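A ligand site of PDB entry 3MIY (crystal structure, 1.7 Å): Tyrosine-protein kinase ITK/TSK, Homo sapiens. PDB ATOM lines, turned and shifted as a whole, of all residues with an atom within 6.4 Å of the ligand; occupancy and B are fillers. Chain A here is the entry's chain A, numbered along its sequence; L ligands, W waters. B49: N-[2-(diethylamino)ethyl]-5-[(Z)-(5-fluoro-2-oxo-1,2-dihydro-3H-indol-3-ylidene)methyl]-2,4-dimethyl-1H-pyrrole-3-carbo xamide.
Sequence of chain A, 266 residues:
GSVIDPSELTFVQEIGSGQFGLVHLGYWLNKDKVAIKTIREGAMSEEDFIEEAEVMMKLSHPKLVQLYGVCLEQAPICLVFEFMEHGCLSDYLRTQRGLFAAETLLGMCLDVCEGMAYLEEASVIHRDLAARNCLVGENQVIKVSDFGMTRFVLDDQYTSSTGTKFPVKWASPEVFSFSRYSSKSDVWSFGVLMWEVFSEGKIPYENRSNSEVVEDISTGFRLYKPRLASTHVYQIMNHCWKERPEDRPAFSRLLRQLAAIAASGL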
ATOM      1  N   ILE A  15     -11.478 -25.861  -9.127  1.00  0.00           N
ATOM      2  CA  ILE A  15     -10.307 -26.193  -9.960  1.00  0.00           C
ATOM      3  C   ILE A  15      -9.631 -24.966 -10.569  1.00  0.00           C
ATOM      4  O   ILE A  15      -8.482 -25.046 -11.014  1.00  0.00           O
ATOM      5  CB  ILE A  15     -10.649 -27.216 -11.072  1.00  0.00           C
ATOM      6  CG1 ILE A  15     -11.850 -26.746 -11.908  1.00  0.00           C
ATOM      7  CG2 ILE A  15     -10.877 -28.609 -10.485  1.00  0.00           C
ATOM      8  CD1 ILE A  15     -12.129 -27.571 -13.153  1.00  0.00           C
ATOM      9  N   GLY A  16     -10.340 -23.836 -10.583  1.00  0.00           N
ATOM     10  CA  GLY A  16      -9.823 -22.608 -11.179  1.00  0.00           C
ATOM     11  C   GLY A  16     -10.112 -21.363 -10.360  1.00  0.00           C
ATOM     12  O   GLY A  16     -10.971 -21.369  -9.470  1.00  0.00           O
ATOM     13  N   VAL A  23     -13.917 -21.496 -11.241  1.00  0.00           N
ATOM     14  CA  VAL A  23     -14.210 -22.682 -12.047  1.00  0.00           C
ATOM     15  C   VAL A  23     -14.319 -23.923 -11.147  1.00  0.00           C
ATOM     16  O   VAL A  23     -13.449 -24.178 -10.322  1.00  0.00           O
ATOM     17  CB  VAL A  23     -13.161 -22.905 -13.168  1.00  0.00           C
ATOM     18  CG1 VAL A  23     -13.546 -24.090 -14.052  1.00  0.00           C
ATOM     19  CG2 VAL A  23     -13.002 -21.656 -14.017  1.00  0.00           C
ATOM     20  N   LEU A  25     -15.191 -28.233 -11.038  1.00  0.00           N
ATOM     21  CA  LEU A  25     -15.440 -29.525 -11.647  1.00  0.00           C
ATOM     22  C   LEU A  25     -16.803 -30.014 -11.151  1.00  0.00           C
ATOM     23  O   LEU A  25     -17.087 -29.979  -9.952  1.00  0.00           O
ATOM     24  CB  LEU A  25     -14.345 -30.533 -11.273  1.00  0.00           C
ATOM     25  CG  LEU A  25     -14.384 -32.009 -11.703  1.00  0.00           C
ATOM     26  CD1 LEU A  25     -15.221 -32.896 -10.788  1.00  0.00           C
ATOM     27  CD2 LEU A  25     -14.815 -32.188 -13.152  1.00  0.00           C
ATOM     28  N   VAL A  34     -18.605 -31.712 -16.404  1.00  0.00           N
ATOM     29  CA  VAL A  34     -18.624 -30.316 -16.839  1.00  0.00           C
ATOM     30  C   VAL A  34     -17.678 -29.432 -16.028  1.00  0.00           C
ATOM     31  O   VAL A  34     -17.301 -29.774 -14.900  1.00  0.00           O
ATOM     32  CB  VAL A  34     -20.049 -29.692 -16.809  1.00  0.00           C
ATOM     33  CG1 VAL A  34     -20.977 -30.394 -17.800  1.00  0.00           C
ATOM     34  CG2 VAL A  34     -20.644 -29.716 -15.389  1.00  0.00           C
ATOM     35  N   ALA A  35     -17.285 -28.313 -16.623  1.00  0.00           N
ATOM     36  CA  ALA A  35     -16.569 -27.264 -15.901  1.00  0.00           C
ATOM     37  C   ALA A  35     -17.530 -26.106 -15.735  1.00  0.00           C
ATOM     38  O   ALA A  35     -17.999 -25.529 -16.720  1.00  0.00           O
ATOM     39  CB  ALA A  35     -15.329 -26.842 -16.645  1.00  0.00           C
ATOM     40  N   LYS A  37     -18.394 -22.384 -14.541  1.00  0.00           N
ATOM     41  CA  LYS A  37     -17.785 -21.088 -14.269  1.00  0.00           C
ATOM     42  C   LYS A  37     -18.792 -20.132 -13.642  1.00  0.00           C
ATOM     43  O   LYS A  37     -19.730 -19.680 -14.304  1.00  0.00           O
ATOM     44  CB  LYS A  37     -17.205 -20.477 -15.553  1.00  0.00           C
ATOM     45  CG  LYS A  37     -16.423 -19.196 -15.309  1.00  0.00           C
ATOM     46  CD  LYS A  37     -16.100 -18.454 -16.588  1.00  0.00           C
ATOM     47  CE  LYS A  37     -14.914 -19.059 -17.307  1.00  0.00           C
ATOM     48  NZ  LYS A  37     -14.554 -18.258 -18.496  1.00  0.00           N
ATOM     49  N   VAL A  65     -13.831 -24.035 -27.480  1.00  0.00           N
ATOM     50  CA  VAL A  65     -14.550 -24.694 -26.384  1.00  0.00           C
ATOM     51  C   VAL A  65     -16.072 -24.499 -26.518  1.00  0.00           C
ATOM     52  O   VAL A  65     -16.532 -23.484 -27.054  1.00  0.00           O
ATOM     53  CB  VAL A  65     -14.012 -24.257 -24.984  1.00  0.00           C
ATOM     54  CG1 VAL A  65     -14.518 -22.880 -24.587  1.00  0.00           C
ATOM     55  CG2 VAL A  65     -14.365 -25.299 -23.912  1.00  0.00           C
ATOM     56  N   GLN A  66     -16.825 -25.494 -26.047  1.00  0.00           N
ATOM     57  CA  GLN A  66     -18.286 -25.486 -26.164  1.00  0.00           C
ATOM     58  C   GLN A  66     -18.965 -25.489 -24.797  1.00  0.00           C
ATOM     59  O   GLN A  66     -18.401 -25.978 -23.818  1.00  0.00           O
ATOM     60  CB  GLN A  66     -18.772 -26.683 -26.966  1.00  0.00           C
ATOM     61  CG  GLN A  66     -18.198 -26.784 -28.369  1.00  0.00           C
ATOM     62  CD  GLN A  66     -18.937 -27.798 -29.194  1.00  0.00           C
ATOM     63  OE1 GLN A  66     -19.763 -27.446 -30.044  1.00  0.00           O
ATOM     64  NE2 GLN A  66     -18.671 -29.069 -28.947  1.00  0.00           N
ATOM     65  N   PHE A  81     -19.707 -25.454 -19.045  1.00  0.00           N
ATOM     66  CA  PHE A  81     -18.843 -25.800 -20.184  1.00  0.00           C
ATOM     67  C   PHE A  81     -18.592 -27.293 -20.243  1.00  0.00           C
ATOM     68  O   PHE A  81     -18.716 -27.992 -19.243  1.00  0.00           O
ATOM     69  CB  PHE A  81     -17.479 -25.107 -20.038  1.00  0.00           C
ATOM     70  CG  PHE A  81     -17.503 -23.623 -20.294  1.00  0.00           C
ATOM     71  CD1 PHE A  81     -17.724 -22.730 -19.251  1.00  0.00           C
ATOM     72  CD2 PHE A  81     -17.269 -23.126 -21.572  1.00  0.00           C
ATOM     73  CE1 PHE A  81     -17.713 -21.363 -19.476  1.00  0.00           C
ATOM     74  CE2 PHE A  81     -17.256 -21.750 -21.809  1.00  0.00           C
ATOM     75  CZ  PHE A  81     -17.484 -20.873 -20.760  1.00  0.00           C
ATOM     76  N   GLU A  82     -18.200 -27.763 -21.432  1.00  0.00           N
ATOM     77  CA  GLU A  82     -17.656 -29.105 -21.559  1.00  0.00           C
ATOM     78  C   GLU A  82     -16.385 -29.219 -20.711  1.00  0.00           C
ATOM     79  O   GLU A  82     -15.669 -28.235 -20.495  1.00  0.00           O
ATOM     80  CB  GLU A  82     -17.330 -29.431 -23.018  1.00  0.00           C
ATOM     81  CG  GLU A  82     -16.221 -28.573 -23.638  1.00  0.00           C
ATOM     82  CD  GLU A  82     -15.852 -28.999 -25.041  1.00  0.00           C
ATOM     83  OE1 GLU A  82     -15.890 -30.216 -25.330  1.00  0.00           O
ATOM     84  OE2 GLU A  82     -15.517 -28.114 -25.859  1.00  0.00           O
ATOM     85  N   PHE A  83     -16.123 -30.432 -20.218  1.00  0.00           N
ATOM     86  CA  PHE A  83     -14.940 -30.692 -19.410  1.00  0.00           C
ATOM     87  C   PHE A  83     -13.753 -31.007 -20.309  1.00  0.00           C
ATOM     88  O   PHE A  83     -13.850 -31.816 -21.229  1.00  0.00           O
ATOM     89  CB  PHE A  83     -15.217 -31.845 -18.450  1.00  0.00           C
ATOM     90  CG  PHE A  83     -14.088 -32.127 -17.486  1.00  0.00           C
ATOM     91  CD1 PHE A  83     -13.792 -31.244 -16.455  1.00  0.00           C
ATOM     92  CD2 PHE A  83     -13.333 -33.287 -17.615  1.00  0.00           C
ATOM     93  CE1 PHE A  83     -12.762 -31.503 -15.571  1.00  0.00           C
ATOM     94  CE2 PHE A  83     -12.297 -33.554 -16.727  1.00  0.00           C
ATOM     95  CZ  PHE A  83     -12.011 -32.669 -15.706  1.00  0.00           C
ATOM     96  N   MET A  84     -12.643 -30.330 -20.035  1.00  0.00           N
ATOM     97  CA  MET A  84     -11.396 -30.554 -20.760  1.00  0.00           C
ATOM     98  C   MET A  84     -10.394 -31.208 -19.812  1.00  0.00           C
ATOM     99  O   MET A  84      -9.829 -30.548 -18.932  1.00  0.00           O
ATOM    100  CB  MET A  84     -10.864 -29.241 -21.343  1.00  0.00           C
ATOM    101  CG  MET A  84     -11.815 -28.598 -22.355  1.00  0.00           C
ATOM    102  SD  MET A  84     -11.926 -29.521 -23.904  1.00  0.00           S
ATOM    103  CE  MET A  84     -10.424 -28.993 -24.711  1.00  0.00           C
ATOM    104  N   GLU A  85     -10.189 -32.505 -20.013  1.00  0.00           N
ATOM    105  CA  GLU A  85      -9.504 -33.356 -19.028  1.00  0.00           C
ATOM    106  C   GLU A  85      -8.115 -32.920 -18.571  1.00  0.00           C
ATOM    107  O   GLU A  85      -7.736 -33.158 -17.423  1.00  0.00           O
ATOM    108  CB  GLU A  85      -9.505 -34.829 -19.476  1.00  0.00           C
ATOM    109  CG  GLU A  85      -8.847 -35.107 -20.823  1.00  0.00           C
ATOM    110  CD  GLU A  85      -9.081 -36.536 -21.312  1.00  0.00           C
ATOM    111  OE1 GLU A  85     -10.189 -37.074 -21.094  1.00  0.00           O
ATOM    112  OE2 GLU A  85      -8.163 -37.111 -21.924  1.00  0.00           O
ATOM    113  N   HIS A  86      -7.354 -32.282 -19.458  1.00  0.00           N
ATOM    114  CA  HIS A  86      -5.996 -31.854 -19.104  1.00  0.00           C
ATOM    115  C   HIS A  86      -5.890 -30.370 -18.721  1.00  0.00           C
ATOM    116  O   HIS A  86      -4.788 -29.824 -18.588  1.00  0.00           O
ATOM    117  CB  HIS A  86      -4.991 -32.216 -20.206  1.00  0.00           C
ATOM    118  CG  HIS A  86      -4.863 -33.688 -20.441  1.00  0.00           C
ATOM    119  ND1 HIS A  86      -4.395 -34.560 -19.490  1.00  0.00           N
ATOM    120  CD2 HIS A  86      -5.124 -34.439 -21.543  1.00  0.00           C
ATOM    121  CE1 HIS A  86      -4.377 -35.791 -19.979  1.00  0.00           C
ATOM    122  NE2 HIS A  86      -4.816 -35.740 -21.231  1.00  0.00           N
ATOM    123  N   GLY A  87      -7.043 -29.727 -18.530  1.00  0.00           N
ATOM    124  CA  GLY A  87      -7.116 -28.356 -18.029  1.00  0.00           C
ATOM    125  C   GLY A  87      -6.506 -27.278 -18.912  1.00  0.00           C
ATOM    126  O   GLY A  87      -6.466 -27.422 -20.129  1.00  0.00           O
ATOM    127  N   CYS A  88      -6.010 -26.214 -18.278  1.00  0.00           N
ATOM    128  CA  CYS A  88      -5.411 -25.081 -18.992  1.00  0.00           C
ATOM    129  C   CYS A  88      -4.097 -25.469 -19.663  1.00  0.00           C
ATOM    130  O   CYS A  88      -3.298 -26.218 -19.088  1.00  0.00           O
ATOM    131  CB  CYS A  88      -5.164 -23.908 -18.050  1.00  0.00           C
ATOM    132  SG  CYS A  88      -6.676 -23.216 -17.342  1.00  0.00           S
ATOM    133  N   ASP A  91      -0.875 -24.617 -17.673  1.00  0.00           N
ATOM    134  CA  ASP A  91      -0.638 -25.583 -16.598  1.00  0.00           C
ATOM    135  C   ASP A  91      -0.133 -26.912 -17.131  1.00  0.00           C
ATOM    136  O   ASP A  91       0.813 -27.489 -16.594  1.00  0.00           O
ATOM    137  CB  ASP A  91      -1.909 -25.795 -15.767  1.00  0.00           C
ATOM    138  CG  ASP A  91      -2.305 -24.571 -14.973  1.00  0.00           C
ATOM    139  OD1 ASP A  91      -1.419 -23.767 -14.617  1.00  0.00           O
ATOM    140  OD2 ASP A  91      -3.514 -24.398 -14.699  1.00  0.00           O
ATOM    141  N   TYR A  92      -0.785 -27.398 -18.196  1.00  0.00           N
ATOM    142  CA  TYR A  92      -0.427 -28.659 -18.835  1.00  0.00           C
ATOM    143  C   TYR A  92       1.011 -28.664 -19.365  1.00  0.00           C
ATOM    144  O   TYR A  92       1.726 -29.663 -19.210  1.00  0.00           O
ATOM    145  CB  TYR A  92      -1.420 -28.987 -19.959  1.00  0.00           C
ATOM    146  CG  TYR A  92      -1.210 -30.333 -20.618  1.00  0.00           C
ATOM    147  CD1 TYR A  92      -1.479 -31.514 -19.923  1.00  0.00           C
ATOM    148  CD2 TYR A  92      -0.739 -30.428 -21.924  1.00  0.00           C
ATOM    149  CE1 TYR A  92      -1.291 -32.763 -20.517  1.00  0.00           C
ATOM    150  CE2 TYR A  92      -0.555 -31.675 -22.535  1.00  0.00           C
ATOM    151  CZ  TYR A  92      -0.831 -32.828 -21.830  1.00  0.00           C
ATOM    152  OH  TYR A  92      -0.646 -34.057 -22.409  1.00  0.00           O
ATOM    153  N   LEU A 135      -7.357 -24.619 -23.577  1.00  0.00           N
ATOM    154  CA  LEU A 135      -7.669 -25.811 -22.800  1.00  0.00           C
ATOM    155  C   LEU A 135      -7.224 -27.064 -23.536  1.00  0.00           C
ATOM    156  O   LEU A 135      -7.223 -27.094 -24.760  1.00  0.00           O
ATOM    157  CB  LEU A 135      -9.162 -25.875 -22.506  1.00  0.00           C
ATOM    158  CG  LEU A 135      -9.734 -24.738 -21.674  1.00  0.00           C
ATOM    159  CD1 LEU A 135     -11.219 -24.633 -21.927  1.00  0.00           C
ATOM    160  CD2 LEU A 135      -9.445 -24.954 -20.187  1.00  0.00           C
ATOM    161  N   VAL A 136      -6.855 -28.085 -22.765  1.00  0.00           N
ATOM    162  CA  VAL A 136      -6.305 -29.317 -23.322  1.00  0.00           C
ATOM    163  C   VAL A 136      -7.271 -30.450 -23.015  1.00  0.00           C
ATOM    164  O   VAL A 136      -7.573 -30.725 -21.854  1.00  0.00           O
ATOM    165  CB  VAL A 136      -4.917 -29.643 -22.731  1.00  0.00           C
ATOM    166  CG1 VAL A 136      -4.276 -30.810 -23.486  1.00  0.00           C
ATOM    167  CG2 VAL A 136      -4.012 -28.426 -22.773  1.00  0.00           C
ATOM    168  N   SER A 145     -10.377 -20.867 -25.372  1.00  0.00           N
ATOM    169  CA  SER A 145     -11.433 -20.550 -24.414  1.00  0.00           C
ATOM    170  C   SER A 145     -11.576 -19.030 -24.271  1.00  0.00           C
ATOM    171  O   SER A 145     -10.726 -18.273 -24.768  1.00  0.00           O
ATOM    172  CB  SER A 145     -11.120 -21.169 -23.051  1.00  0.00           C
ATOM    173  OG  SER A 145     -12.212 -21.057 -22.162  1.00  0.00           O
ATOM    174  N   ASP A 146     -12.638 -18.602 -23.599  1.00  0.00           N
ATOM    175  CA  ASP A 146     -12.875 -17.196 -23.271  1.00  0.00           C
ATOM    176  C   ASP A 146     -12.771 -16.243 -24.463  1.00  0.00           C
ATOM    177  O   ASP A 146     -12.108 -15.197 -24.389  1.00  0.00           O
ATOM    178  CB  ASP A 146     -11.957 -16.746 -22.116  1.00  0.00           C
ATOM    179  CG  ASP A 146     -12.321 -17.401 -20.794  1.00  0.00           C
ATOM    180  OD1 ASP A 146     -13.365 -18.075 -20.719  1.00  0.00           O
ATOM    181  OD2 ASP A 146     -11.550 -17.236 -19.817  1.00  0.00           O
HETATM  182  C4  B49 L   1      -9.197 -30.523 -15.533  1.00  0.00           C
HETATM  183  C5  B49 L   1     -14.077 -23.243 -19.808  1.00  0.00           C
HETATM  184  C6  B49 L   1     -14.171 -24.610 -20.006  1.00  0.00           C
HETATM  185  C7  B49 L   1     -12.414 -23.581 -18.109  1.00  0.00           C
HETATM  186  C13 B49 L   1      -9.165 -26.820 -15.097  1.00  0.00           C
HETATM  187  C15 B49 L   1     -13.195 -22.728 -18.863  1.00  0.00           C
HETATM  188  C17 B49 L   1     -12.510 -24.957 -18.296  1.00  0.00           C
HETATM  189  C20 B49 L   1     -11.823 -26.106 -17.682  1.00  0.00           C
HETATM  190  C21 B49 L   1     -12.397 -27.304 -18.344  1.00  0.00           C
HETATM  191  C22 B49 L   1      -7.634 -28.388 -13.711  1.00  0.00           C
HETATM  192  C3  B49 L   1      -8.763 -25.484 -14.527  1.00  0.00           C
HETATM  193  C12 B49 L   1     -10.842 -25.980 -16.702  1.00  0.00           C
HETATM  194  C14 B49 L   1      -9.353 -29.028 -15.521  1.00  0.00           C
HETATM  195  C16 B49 L   1     -13.388 -25.482 -19.266  1.00  0.00           C
HETATM  196  C18 B49 L   1     -10.117 -27.017 -16.074  1.00  0.00           C
HETATM  197  C19 B49 L   1      -8.671 -28.102 -14.739  1.00  0.00           C
HETATM  198  N23 B49 L   1     -10.208 -28.369 -16.324  1.00  0.00           N
HETATM  199  N24 B49 L   1     -13.289 -26.868 -19.247  1.00  0.00           N
HETATM  200  N25 B49 L   1      -7.628 -29.572 -13.056  1.00  0.00           N
HETATM  201  O27 B49 L   1     -12.142 -28.471 -18.134  1.00  0.00           O
HETATM  202  O28 B49 L   1      -6.792 -27.544 -13.449  1.00  0.00           O
HETATM  203  F29 B49 L   1     -13.115 -21.394 -18.686  1.00  0.00           F
HETATM  204  C37 B49 L   1      -6.620 -29.879 -12.032  1.00  0.00           C
HETATM  205  C38 B49 L   1      -5.383 -30.490 -12.702  1.00  0.00           C
HETATM  206  N4  B49 L   1      -5.558 -31.945 -12.837  1.00  0.00           N
HETATM  207  C39 B49 L   1      -5.898 -32.426 -14.202  1.00  0.00           C
HETATM  208  C40 B49 L   1      -4.440 -32.691 -12.242  1.00  0.00           C
HETATM  209  C41 B49 L   1      -4.931 -33.451 -11.006  1.00  0.00           C
HETATM  210  C42 B49 L   1      -5.320 -31.560 -15.321  1.00  0.00           C
HETATM  211  O   HOH W   1      -3.481 -28.851 -16.510  1.00  0.00           O
HETATM  212  O   HOH W   2      -9.520 -31.638 -12.285  1.00  0.00           O
HETATM  213  O   HOH W   3      -5.241 -26.487 -15.584  1.00  0.00           O
HETATM  214  O   HOH W   4      -3.404 -33.798 -17.022  1.00  0.00           O
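OE2 of Glu 82 is in hydrogen-bond range of N of Gln 66, at 2.9 Å. The side-chain amino group (NZ) of Lys 37 is in salt-bridge range of the side-chain carboxylate (OD1) of Asp 146, 2.5 Å away. The backbone carbonyl oxygen of Ala 35 sits at hydrogen-bond distance from the backbone NH of Phe 81. The backbone carbonyl oxygen of Gly 87 sits at hydrogen-bond distance from the backbone NH of Val 136 (2.7 Å). The backbone NH (N) of Ile 15 sits at hydrogen-bond distance from the backbone carbonyl oxygen (O) of Val 23 (2.9 Å). The backbone NH (N) of His 86 sits at hydrogen-bond distance from the backbone carbonyl oxygen (O) of Val 136.
Water W3 lies within hydrogen-bond range of the backbone NH of Cys 88 (2.8 Å), an oxygen (O28) of the ligand (2.8 Å) and the side-chain carboxylate of Asp 91 (2.9 Å). Water W1 lies within hydrogen-bond range of the backbone carbonyl oxygen (O) of His 86 and the backbone NH (N) of Tyr 92.
F29 of the ligand lies close to NZ of Lys 37 (3.5 Å). O of Ile 15 touches C3 of the ligand, 3.6 Å away. Ala 35 touches the ligand. Val 65 touches the ligand. Phe 81 touches the ligand. Phe 83 touches the ligand. Glu 85 touches the ligand. His 86 touches the ligand (C to C42, 3.6 Å). CA of Gly 87 touches C14 of the ligand, 3.4 Å away. Leu 135 touches the ligand. Ser 145 touches the ligand (OG to F29, 3.6 Å). OD1 of Asp 146 touches F29 of the ligand (3.9 Å). Of the 23 residues printed, 14 come within 4 Å of the ligand. The nearest printed residue that does not touch the ligand is Cys 88 (4.2 Å).
O27 of the ligand lies within hydrogen-bond range of N of Met 84, at 2.7 Å. The backbone carbonyl oxygen (O) of Met 84 lies within hydrogen-bond range of a nitrogen (N23) of the ligand (3.4 Å). A nitrogen (N24) of the ligand sits at hydrogen-bond distance from the backbone carbonyl oxygen (O) of Glu 82, 3.0 Å away.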
